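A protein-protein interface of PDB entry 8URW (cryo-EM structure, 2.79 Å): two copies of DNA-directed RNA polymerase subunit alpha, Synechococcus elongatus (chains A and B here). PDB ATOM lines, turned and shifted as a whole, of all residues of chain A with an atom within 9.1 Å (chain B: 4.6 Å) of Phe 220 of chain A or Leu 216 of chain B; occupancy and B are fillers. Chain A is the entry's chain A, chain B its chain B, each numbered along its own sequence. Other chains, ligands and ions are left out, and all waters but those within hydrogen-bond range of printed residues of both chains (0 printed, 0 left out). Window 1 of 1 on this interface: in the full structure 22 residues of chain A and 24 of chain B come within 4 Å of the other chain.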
ATOM      1  N   MET A   1      10.378 -14.268   7.292  1.00  0.00           N
ATOM      2  CA  MET A   1      10.245 -13.192   8.267  1.00  0.00           C
ATOM      3  C   MET A   1       8.838 -12.573   8.224  1.00  0.00           C
ATOM      4  O   MET A   1       8.234 -12.343   9.271  1.00  0.00           O
ATOM      5  CB  MET A   1      11.363 -12.152   8.049  1.00  0.00           C
ATOM      6  CG  MET A   1      11.118 -11.113   6.965  1.00  0.00           C
ATOM      7  SD  MET A   1      11.144 -11.857   5.319  1.00  0.00           S
ATOM      8  CE  MET A   1      10.915 -10.419   4.277  1.00  0.00           C
ATOM      9  N   PHE A   3       5.267 -13.613   6.107  1.00  0.00           N
ATOM     10  CA  PHE A   3       4.665 -14.547   5.169  1.00  0.00           C
ATOM     11  C   PHE A   3       3.183 -14.680   5.491  1.00  0.00           C
ATOM     12  O   PHE A   3       2.680 -14.104   6.460  1.00  0.00           O
ATOM     13  CB  PHE A   3       5.374 -15.907   5.203  1.00  0.00           C
ATOM     14  CG  PHE A   3       5.536 -16.480   6.582  1.00  0.00           C
ATOM     15  CD1 PHE A   3       4.498 -17.170   7.185  1.00  0.00           C
ATOM     16  CD2 PHE A   3       6.728 -16.335   7.271  1.00  0.00           C
ATOM     17  CE1 PHE A   3       4.645 -17.702   8.452  1.00  0.00           C
ATOM     18  CE2 PHE A   3       6.881 -16.862   8.538  1.00  0.00           C
ATOM     19  CZ  PHE A   3       5.839 -17.548   9.129  1.00  0.00           C
ATOM     20  N   GLN A  31      14.374 -23.141   4.172  1.00  0.00           N
ATOM     21  CA  GLN A  31      13.693 -23.018   5.455  1.00  0.00           C
ATOM     22  C   GLN A  31      12.427 -23.860   5.548  1.00  0.00           C
ATOM     23  O   GLN A  31      11.897 -24.026   6.654  1.00  0.00           O
ATOM     24  CB  GLN A  31      13.359 -21.551   5.724  1.00  0.00           C
ATOM     25  CG  GLN A  31      14.579 -20.682   5.966  1.00  0.00           C
ATOM     26  CD  GLN A  31      14.219 -19.268   6.367  1.00  0.00           C
ATOM     27  OE1 GLN A  31      13.143 -18.771   6.033  1.00  0.00           O
ATOM     28  NE2 GLN A  31      15.120 -18.609   7.082  1.00  0.00           N
ATOM     29  N   THR A  34      13.245 -26.863   7.582  1.00  0.00           N
ATOM     30  CA  THR A  34      13.530 -26.435   8.947  1.00  0.00           C
ATOM     31  C   THR A  34      12.248 -26.182   9.729  1.00  0.00           C
ATOM     32  O   THR A  34      12.135 -26.583  10.893  1.00  0.00           O
ATOM     33  CB  THR A  34      14.399 -25.176   8.926  1.00  0.00           C
ATOM     34  OG1 THR A  34      15.575 -25.415   8.142  1.00  0.00           O
ATOM     35  CG2 THR A  34      14.812 -24.786  10.335  1.00  0.00           C
ATOM     36  N   VAL A  35      11.272 -25.516   9.111  1.00  0.00           N
ATOM     37  CA  VAL A  35      10.005 -25.270   9.793  1.00  0.00           C
ATOM     38  C   VAL A  35       9.201 -26.561   9.923  1.00  0.00           C
ATOM     39  O   VAL A  35       8.672 -26.878  10.997  1.00  0.00           O
ATOM     40  CB  VAL A  35       9.208 -24.176   9.059  1.00  0.00           C
ATOM     41  CG1 VAL A  35       7.843 -23.994   9.698  1.00  0.00           C
ATOM     42  CG2 VAL A  35       9.978 -22.867   9.064  1.00  0.00           C
ATOM     43  N   ALA A  38      10.498 -29.394  12.509  1.00  0.00           N
ATOM     44  CA  ALA A  38      10.288 -28.958  13.885  1.00  0.00           C
ATOM     45  C   ALA A  38       8.813 -29.002  14.256  1.00  0.00           C
ATOM     46  O   ALA A  38       8.453 -29.466  15.347  1.00  0.00           O
ATOM     47  CB  ALA A  38      10.850 -27.550  14.081  1.00  0.00           C
ATOM     48  N   LEU A  39       7.941 -28.533  13.357  1.00  0.00           N
ATOM     49  CA  LEU A  39       6.510 -28.572  13.644  1.00  0.00           C
ATOM     50  C   LEU A  39       6.023 -30.006  13.819  1.00  0.00           C
ATOM     51  O   LEU A  39       5.259 -30.296  14.746  1.00  0.00           O
ATOM     52  CB  LEU A  39       5.729 -27.869  12.536  1.00  0.00           C
ATOM     53  CG  LEU A  39       5.651 -26.343  12.618  1.00  0.00           C
ATOM     54  CD1 LEU A  39       5.015 -25.773  11.362  1.00  0.00           C
ATOM     55  CD2 LEU A  39       4.885 -25.906  13.852  1.00  0.00           C
ATOM     56  N   VAL A  42       7.353 -31.461  17.231  1.00  0.00           N
ATOM     57  CA  VAL A  42       6.668 -30.911  18.396  1.00  0.00           C
ATOM     58  C   VAL A  42       5.223 -31.395  18.448  1.00  0.00           C
ATOM     59  O   VAL A  42       4.699 -31.711  19.523  1.00  0.00           O
ATOM     60  CB  VAL A  42       6.760 -29.375  18.389  1.00  0.00           C
ATOM     61  CG1 VAL A  42       5.837 -28.778  19.433  1.00  0.00           C
ATOM     62  CG2 VAL A  42       8.189 -28.940  18.639  1.00  0.00           C
ATOM     63  N   ALA A 212       1.586 -25.871  19.234  1.00  0.00           N
ATOM     64  CA  ALA A 212       2.942 -26.231  18.829  1.00  0.00           C
ATOM     65  C   ALA A 212       3.795 -24.992  18.583  1.00  0.00           C
ATOM     66  O   ALA A 212       4.964 -24.942  18.990  1.00  0.00           O
ATOM     67  CB  ALA A 212       2.900 -27.112  17.581  1.00  0.00           C
ATOM     68  N   ALA A 213       3.229 -23.981  17.918  1.00  0.00           N
ATOM     69  CA  ALA A 213       3.976 -22.750  17.675  1.00  0.00           C
ATOM     70  C   ALA A 213       4.337 -22.056  18.982  1.00  0.00           C
ATOM     71  O   ALA A 213       5.455 -21.548  19.136  1.00  0.00           O
ATOM     72  CB  ALA A 213       3.169 -21.817  16.772  1.00  0.00           C
ATOM     73  N   SER A 214       3.404 -22.024  19.937  1.00  0.00           N
ATOM     74  CA  SER A 214       3.697 -21.419  21.233  1.00  0.00           C
ATOM     75  C   SER A 214       4.812 -22.167  21.952  1.00  0.00           C
ATOM     76  O   SER A 214       5.707 -21.547  22.543  1.00  0.00           O
ATOM     77  CB  SER A 214       2.435 -21.381  22.094  1.00  0.00           C
ATOM     78  OG  SER A 214       1.341 -20.847  21.373  1.00  0.00           O
ATOM     79  N   CYS A 215       4.776 -23.502  21.913  1.00  0.00           N
ATOM     80  CA  CYS A 215       5.828 -24.285  22.553  1.00  0.00           C
ATOM     81  C   CYS A 215       7.187 -24.012  21.918  1.00  0.00           C
ATOM     82  O   CYS A 215       8.191 -23.850  22.623  1.00  0.00           O
ATOM     83  CB  CYS A 215       5.489 -25.774  22.483  1.00  0.00           C
ATOM     84  SG  CYS A 215       6.592 -26.833  23.441  1.00  0.00           S
ATOM     85  N   LEU A 216       7.239 -23.949  20.584  1.00  0.00           N
ATOM     86  CA  LEU A 216       8.508 -23.688  19.911  1.00  0.00           C
ATOM     87  C   LEU A 216       9.039 -22.296  20.237  1.00  0.00           C
ATOM     88  O   LEU A 216      10.247 -22.116  20.450  1.00  0.00           O
ATOM     89  CB  LEU A 216       8.348 -23.863  18.402  1.00  0.00           C
ATOM     90  CG  LEU A 216       8.454 -25.302  17.894  1.00  0.00           C
ATOM     91  CD1 LEU A 216       7.890 -25.426  16.489  1.00  0.00           C
ATOM     92  CD2 LEU A 216       9.896 -25.779  17.940  1.00  0.00           C
ATOM     93  N   VAL A 217       8.154 -21.295  20.273  1.00  0.00           N
ATOM     94  CA  VAL A 217       8.581 -19.941  20.620  1.00  0.00           C
ATOM     95  C   VAL A 217       9.127 -19.903  22.042  1.00  0.00           C
ATOM     96  O   VAL A 217      10.176 -19.299  22.304  1.00  0.00           O
ATOM     97  CB  VAL A 217       7.418 -18.950  20.431  1.00  0.00           C
ATOM     98  CG1 VAL A 217       7.695 -17.653  21.170  1.00  0.00           C
ATOM     99  CG2 VAL A 217       7.193 -18.681  18.955  1.00  0.00           C
ATOM    100  N   ALA A 218       8.429 -20.548  22.981  1.00  0.00           N
ATOM    101  CA  ALA A 218       8.904 -20.585  24.359  1.00  0.00           C
ATOM    102  C   ALA A 218      10.249 -21.293  24.461  1.00  0.00           C
ATOM    103  O   ALA A 218      11.092 -20.925  25.287  1.00  0.00           O
ATOM    104  CB  ALA A 218       7.869 -21.267  25.255  1.00  0.00           C
ATOM    105  N   LEU A 219      10.466 -22.316  23.632  1.00  0.00           N
ATOM    106  CA  LEU A 219      11.752 -23.007  23.637  1.00  0.00           C
ATOM    107  C   LEU A 219      12.875 -22.110  23.133  1.00  0.00           C
ATOM    108  O   LEU A 219      13.945 -22.041  23.749  1.00  0.00           O
ATOM    109  CB  LEU A 219      11.674 -24.274  22.785  1.00  0.00           C
ATOM    110  CG  LEU A 219      11.608 -25.614  23.515  1.00  0.00           C
ATOM    111  CD1 LEU A 219      11.527 -26.753  22.514  1.00  0.00           C
ATOM    112  CD2 LEU A 219      12.812 -25.782  24.424  1.00  0.00           C
ATOM    113  N   PHE A 220      12.656 -21.417  22.018  1.00  0.00           N
ATOM    114  CA  PHE A 220      13.727 -20.677  21.361  1.00  0.00           C
ATOM    115  C   PHE A 220      13.878 -19.243  21.853  1.00  0.00           C
ATOM    116  O   PHE A 220      14.788 -18.544  21.395  1.00  0.00           O
ATOM    117  CB  PHE A 220      13.516 -20.676  19.844  1.00  0.00           C
ATOM    118  CG  PHE A 220      13.930 -21.954  19.179  1.00  0.00           C
ATOM    119  CD1 PHE A 220      15.254 -22.360  19.195  1.00  0.00           C
ATOM    120  CD2 PHE A 220      12.998 -22.750  18.538  1.00  0.00           C
ATOM    121  CE1 PHE A 220      15.639 -23.536  18.586  1.00  0.00           C
ATOM    122  CE2 PHE A 220      13.376 -23.927  17.927  1.00  0.00           C
ATOM    123  CZ  PHE A 220      14.698 -24.320  17.951  1.00  0.00           C
ATOM    124  N   GLU A 221      13.027 -18.780  22.765  1.00  0.00           N
ATOM    125  CA  GLU A 221      13.136 -17.400  23.229  1.00  0.00           C
ATOM    126  C   GLU A 221      14.316 -17.151  24.171  1.00  0.00           C
ATOM    127  O   GLU A 221      15.050 -16.176  23.966  1.00  0.00           O
ATOM    128  CB  GLU A 221      11.834 -16.956  23.899  1.00  0.00           C
ATOM    129  CG  GLU A 221      11.862 -15.513  24.367  1.00  0.00           C
ATOM    130  CD  GLU A 221      10.643 -14.732  23.925  1.00  0.00           C
ATOM    131  OE1 GLU A 221      10.794 -13.817  23.088  1.00  0.00           O
ATOM    132  OE2 GLU A 221       9.535 -15.032  24.413  1.00  0.00           O
ATOM    133  N   PRO A 222      14.550 -17.973  25.204  1.00  0.00           N
ATOM    134  CA  PRO A 222      15.581 -17.622  26.195  1.00  0.00           C
ATOM    135  C   PRO A 222      17.014 -17.682  25.686  1.00  0.00           C
ATOM    136  O   PRO A 222      17.938 -17.478  26.483  1.00  0.00           O
ATOM    137  CB  PRO A 222      15.364 -18.659  27.310  1.00  0.00           C
ATOM    138  CG  PRO A 222      13.991 -19.171  27.100  1.00  0.00           C
ATOM    139  CD  PRO A 222      13.815 -19.178  25.623  1.00  0.00           C
ATOM    140  N   LEU A 223      17.247 -17.952  24.404  1.00  0.00           N
ATOM    141  CA  LEU A 223      18.599 -18.009  23.864  1.00  0.00           C
ATOM    142  C   LEU A 223      19.053 -16.693  23.245  1.00  0.00           C
ATOM    143  O   LEU A 223      20.174 -16.623  22.730  1.00  0.00           O
ATOM    144  CB  LEU A 223      18.705 -19.128  22.821  1.00  0.00           C
ATOM    145  CG  LEU A 223      18.642 -20.567  23.335  1.00  0.00           C
ATOM    146  CD1 LEU A 223      18.353 -21.529  22.194  1.00  0.00           C
ATOM    147  CD2 LEU A 223      19.932 -20.944  24.042  1.00  0.00           C
ATOM    148  N   LYS A 224      18.220 -15.657  23.278  1.00  0.00           N
ATOM    149  CA  LYS A 224      18.534 -14.380  22.652  1.00  0.00           C
ATOM    150  C   LYS A 224      19.240 -13.404  23.585  1.00  0.00           C
ATOM    151  O   LYS A 224      19.586 -12.301  23.150  1.00  0.00           O
ATOM    152  CB  LYS A 224      17.256 -13.723  22.126  1.00  0.00           C
ATOM    153  CG  LYS A 224      16.568 -14.481  21.008  1.00  0.00           C
ATOM    154  CD  LYS A 224      15.083 -14.161  20.968  1.00  0.00           C
ATOM    155  CE  LYS A 224      14.826 -12.676  21.157  1.00  0.00           C
ATOM    156  NZ  LYS A 224      14.510 -11.995  19.873  1.00  0.00           N
ATOM    157  N   ASN A 225      19.463 -13.772  24.846  1.00  0.00           N
ATOM    158  CA  ASN A 225      19.939 -12.809  25.835  1.00  0.00           C
ATOM    159  C   ASN A 225      21.461 -12.681  25.830  1.00  0.00           C
ATOM    160  O   ASN A 225      21.998 -11.597  25.578  1.00  0.00           O
ATOM    161  CB  ASN A 225      19.436 -13.205  27.228  1.00  0.00           C
ATOM    162  CG  ASN A 225      17.944 -13.472  27.253  1.00  0.00           C
ATOM    163  OD1 ASN A 225      17.153 -12.688  26.726  1.00  0.00           O
ATOM    164  ND2 ASN A 225      17.550 -14.580  27.867  1.00  0.00           N
ATOM    165  N   SER A 227      23.778 -15.981  25.239  1.00  0.00           N
ATOM    166  CA  SER A 227      24.248 -17.013  24.326  1.00  0.00           C
ATOM    167  C   SER A 227      23.245 -18.158  24.254  1.00  0.00           C
ATOM    168  O   SER A 227      22.050 -17.962  24.474  1.00  0.00           O
ATOM    169  CB  SER A 227      25.618 -17.535  24.760  1.00  0.00           C
ATOM    170  OG  SER A 227      25.720 -17.584  26.173  1.00  0.00           O
ATOM    171  N   VAL B  35      16.057 -28.991  18.894  1.00  0.00           N
ATOM    172  CA  VAL B  35      16.724 -27.716  19.146  1.00  0.00           C
ATOM    173  C   VAL B  35      18.084 -27.685  18.459  1.00  0.00           C
ATOM    174  O   VAL B  35      18.429 -26.717  17.769  1.00  0.00           O
ATOM    175  CB  VAL B  35      16.847 -27.465  20.661  1.00  0.00           C
ATOM    176  CG1 VAL B  35      17.804 -26.322  20.934  1.00  0.00           C
ATOM    177  CG2 VAL B  35      15.482 -27.171  21.257  1.00  0.00           C
ATOM    178  N   ALA B  38      17.699 -27.580  14.490  1.00  0.00           N
ATOM    179  CA  ALA B  38      17.257 -26.269  14.024  1.00  0.00           C
ATOM    180  C   ALA B  38      18.363 -25.233  14.168  1.00  0.00           C
ATOM    181  O   ALA B  38      18.598 -24.431  13.252  1.00  0.00           O
ATOM    182  CB  ALA B  38      16.009 -25.832  14.788  1.00  0.00           C
ATOM    183  N   LEU B  39      19.069 -25.246  15.304  1.00  0.00           N
ATOM    184  CA  LEU B  39      20.150 -24.289  15.504  1.00  0.00           C
ATOM    185  C   LEU B  39      21.260 -24.489  14.483  1.00  0.00           C
ATOM    186  O   LEU B  39      21.777 -23.515  13.928  1.00  0.00           O
ATOM    187  CB  LEU B  39      20.697 -24.405  16.926  1.00  0.00           C
ATOM    188  CG  LEU B  39      19.885 -23.698  18.013  1.00  0.00           C
ATOM    189  CD1 LEU B  39      20.418 -24.046  19.393  1.00  0.00           C
ATOM    190  CD2 LEU B  39      19.888 -22.196  17.795  1.00  0.00           C
ATOM    191  N   VAL B  42      20.053 -23.261  10.954  1.00  0.00           N
ATOM    192  CA  VAL B  42      19.981 -21.807  10.845  1.00  0.00           C
ATOM    193  C   VAL B  42      21.375 -21.192  10.887  1.00  0.00           C
ATOM    194  O   VAL B  42      21.675 -20.252  10.140  1.00  0.00           O
ATOM    195  CB  VAL B  42      19.068 -21.234  11.943  1.00  0.00           C
ATOM    196  CG1 VAL B  42      19.147 -19.719  11.961  1.00  0.00           C
ATOM    197  CG2 VAL B  42      17.638 -21.681  11.718  1.00  0.00           C
ATOM    198  N   ALA B 212      20.969 -16.440  15.582  1.00  0.00           N
ATOM    199  CA  ALA B 212      20.208 -17.594  15.112  1.00  0.00           C
ATOM    200  C   ALA B 212      18.924 -17.775  15.915  1.00  0.00           C
ATOM    201  O   ALA B 212      17.861 -18.063  15.348  1.00  0.00           O
ATOM    202  CB  ALA B 212      21.068 -18.855  15.182  1.00  0.00           C
ATOM    203  N   ALA B 213      19.004 -17.611  17.239  1.00  0.00           N
ATOM    204  CA  ALA B 213      17.810 -17.733  18.070  1.00  0.00           C
ATOM    205  C   ALA B 213      16.783 -16.664  17.723  1.00  0.00           C
ATOM    206  O   ALA B 213      15.579 -16.944  17.664  1.00  0.00           O
ATOM    207  CB  ALA B 213      18.188 -17.658  19.547  1.00  0.00           C
ATOM    208  N   SER B 214      17.238 -15.430  17.491  1.00  0.00           N
ATOM    209  CA  SER B 214      16.314 -14.368  17.107  1.00  0.00           C
ATOM    210  C   SER B 214      15.652 -14.669  15.769  1.00  0.00           C
ATOM    211  O   SER B 214      14.449 -14.436  15.596  1.00  0.00           O
ATOM    212  CB  SER B 214      17.047 -13.028  17.057  1.00  0.00           C
ATOM    213  OG  SER B 214      17.300 -12.637  15.720  1.00  0.00           O
ATOM    214  N   CYS B 215      16.423 -15.190  14.810  1.00  0.00           N
ATOM    215  CA  CYS B 215      15.848 -15.536  13.512  1.00  0.00           C
ATOM    216  C   CYS B 215      14.792 -16.626  13.651  1.00  0.00           C
ATOM    217  O   CYS B 215      13.719 -16.543  13.044  1.00  0.00           O
ATOM    218  CB  CYS B 215      16.950 -15.973  12.548  1.00  0.00           C
ATOM    219  SG  CYS B 215      16.353 -16.719  11.014  1.00  0.00           S
ATOM    220  N   LEU B 216      15.074 -17.654  14.457  1.00  0.00           N
ATOM    221  CA  LEU B 216      14.097 -18.725  14.651  1.00  0.00           C
ATOM    222  C   LEU B 216      12.839 -18.216  15.350  1.00  0.00           C
ATOM    223  O   LEU B 216      11.719 -18.622  15.003  1.00  0.00           O
ATOM    224  CB  LEU B 216      14.725 -19.872  15.439  1.00  0.00           C
ATOM    225  CG  LEU B 216      15.472 -20.909  14.603  1.00  0.00           C
ATOM    226  CD1 LEU B 216      16.497 -21.643  15.446  1.00  0.00           C
ATOM    227  CD2 LEU B 216      14.497 -21.886  13.973  1.00  0.00           C
ATOM    228  N   VAL B 217      13.000 -17.340  16.346  1.00  0.00           N
ATOM    229  CA  VAL B 217      11.842 -16.784  17.039  1.00  0.00           C
ATOM    230  C   VAL B 217      10.987 -15.966  16.080  1.00  0.00           C
ATOM    231  O   VAL B 217       9.752 -16.061  16.088  1.00  0.00           O
ATOM    232  CB  VAL B 217      12.297 -15.950  18.252  1.00  0.00           C
ATOM    233  CG1 VAL B 217      11.211 -14.976  18.673  1.00  0.00           C
ATOM    234  CG2 VAL B 217      12.668 -16.861  19.407  1.00  0.00           C
ATOM    235  N   ALA B 218      11.626 -15.147  15.241  1.00  0.00           N
ATOM    236  CA  ALA B 218      10.883 -14.377  14.249  1.00  0.00           C
ATOM    237  C   ALA B 218      10.189 -15.292  13.249  1.00  0.00           C
ATOM    238  O   ALA B 218       9.099 -14.976  12.759  1.00  0.00           O
ATOM    239  CB  ALA B 218      11.819 -13.407  13.530  1.00  0.00           C
ATOM    240  N   LEU B 219      10.812 -16.427  12.926  1.00  0.00           N
ATOM    241  CA  LEU B 219      10.188 -17.384  12.017  1.00  0.00           C
ATOM    242  C   LEU B 219       8.930 -17.992  12.620  1.00  0.00           C
ATOM    243  O   LEU B 219       7.902 -18.104  11.942  1.00  0.00           O
ATOM    244  CB  LEU B 219      11.185 -18.484  11.654  1.00  0.00           C
ATOM    245  CG  LEU B 219      11.177 -19.013  10.221  1.00  0.00           C
ATOM    246  CD1 LEU B 219      11.281 -17.874   9.224  1.00  0.00           C
ATOM    247  CD2 LEU B 219      12.305 -20.012  10.024  1.00  0.00           C
ATOM    248  N   PHE B 220       8.989 -18.397  13.887  1.00  0.00           N
ATOM    249  CA  PHE B 220       7.881 -19.129  14.494  1.00  0.00           C
ATOM    250  C   PHE B 220       6.832 -18.242  15.154  1.00  0.00           C
ATOM    251  O   PHE B 220       5.779 -18.757  15.544  1.00  0.00           O
ATOM    252  CB  PHE B 220       8.405 -20.131  15.528  1.00  0.00           C
ATOM    253  CG  PHE B 220       8.985 -21.373  14.924  1.00  0.00           C
ATOM    254  CD1 PHE B 220       8.230 -22.157  14.070  1.00  0.00           C
ATOM    255  CD2 PHE B 220      10.282 -21.760  15.213  1.00  0.00           C
ATOM    256  CE1 PHE B 220       8.757 -23.303  13.512  1.00  0.00           C
ATOM    257  CE2 PHE B 220      10.815 -22.905  14.657  1.00  0.00           C
ATOM    258  CZ  PHE B 220      10.052 -23.678  13.806  1.00  0.00           C
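Gln 31 of chain A touches Leu 219 of chain B (OE1 to CD1, 3.8 Å).
Val 35 of chain A touches Leu 219 of chain B.
Phe 220 of chain B touches Val 35 of chain A (CE1 to CG1, 3.98 Å).
CE1 of Phe 220 of chain B touches CD1 of Leu 216 of chain A (3.8 Å).
O of Phe 220 of chain B touches CG2 of Val 217 of chain A, 3.7 Å away.
Phe 220 of chain A touches Leu 216 of chain B (CE1 to CD1, 3.8 Å).
O of Phe 220 of chain A touches CG2 of Val 217 of chain B (3.4 Å).
Glu 221 of chain A touches Val 217 of chain B.
Leu 223 of chain A touches Ala 213 of chain B (CB to CB, 3.6 Å).
Lys 224 of chain A touches Ser 214 of chain B.
Printed residues of chain B within 4 Å of Phe 3 of chain A: Leu 219.
Printed residues of chain B within 4 Å of Val 217 of chain A: Phe 220 (3.7 Å).
Of the printed residues of chain B, Lys 224 of chain A touches Ala 213, Ser 214 and Val 217.
No residue of chain A comes within 4 Å of Val 35 of chain B.
Of chain A, only Phe 220 (3.4 Å), Glu 221 (3.9 Å) and Lys 224 (3.9 Å) come within 4 Å of Val 217 of chain B.
Of the printed residues of chain A, Phe 220 of chain B touches Val 35 (3.98 Å), Ala 38 (3.96 Å), Leu 216 (3.8 Å) and Val 217 (3.7 Å).
The nearest residue of chain B that does not touch Phe 220 of chain A is Val 35 of chain B (4.1 Å).
Printed residues of chain A that touch a printed residue of chain B: Phe 3, Gln 31, Val 35, Ala 38, Leu 216, Val 217, Phe 220, Glu 221, Leu 223 and Lys 224.
Of the 13 printed residues of chain B, 7 touch a printed residue of chain A.
Hydrophobic or aromatic side chains of chain B within 4 Å of the printed part of chain A: Ala 38, Ala 213, Leu 216, Val 217, Leu 219 and Phe 220.
Among the printed residues, 16 pairs touch across the chains.
Among the printed residues, no Asp or Glu carboxylate lies within 4 Å of a Lys or Arg side-chain nitrogen of the other chain.
Val 35 of chain A touches Phe 220 of chain B, but with the chains exchanged Phe 220 of chain A does not touch Val 35 of chain B (4.1 Å).
Ala 38 of chain A touches Phe 220 of chain B, and with the chains exchanged Phe 220 of chain A touches Ala 38 of chain B.
Val 217 of chain A touches Phe 220 of chain B, and with the chains exchanged Phe 220 of chain A touches Val 217 of chain B.
Phe 220 of chain A touches Ala 213 of chain B, but with the chains exchanged Ala 213 of chain A does not touch Phe 220 of chain B (4.2 Å).
Positions printed for both chains: 35, 38, 39, 42, 212, 213, 214, 215, 216, 217, 218, 219 and 220.
Of the 16 pairs that touch across the chains among the printed residues, 6 have their exchanged pair printed and touching as well.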
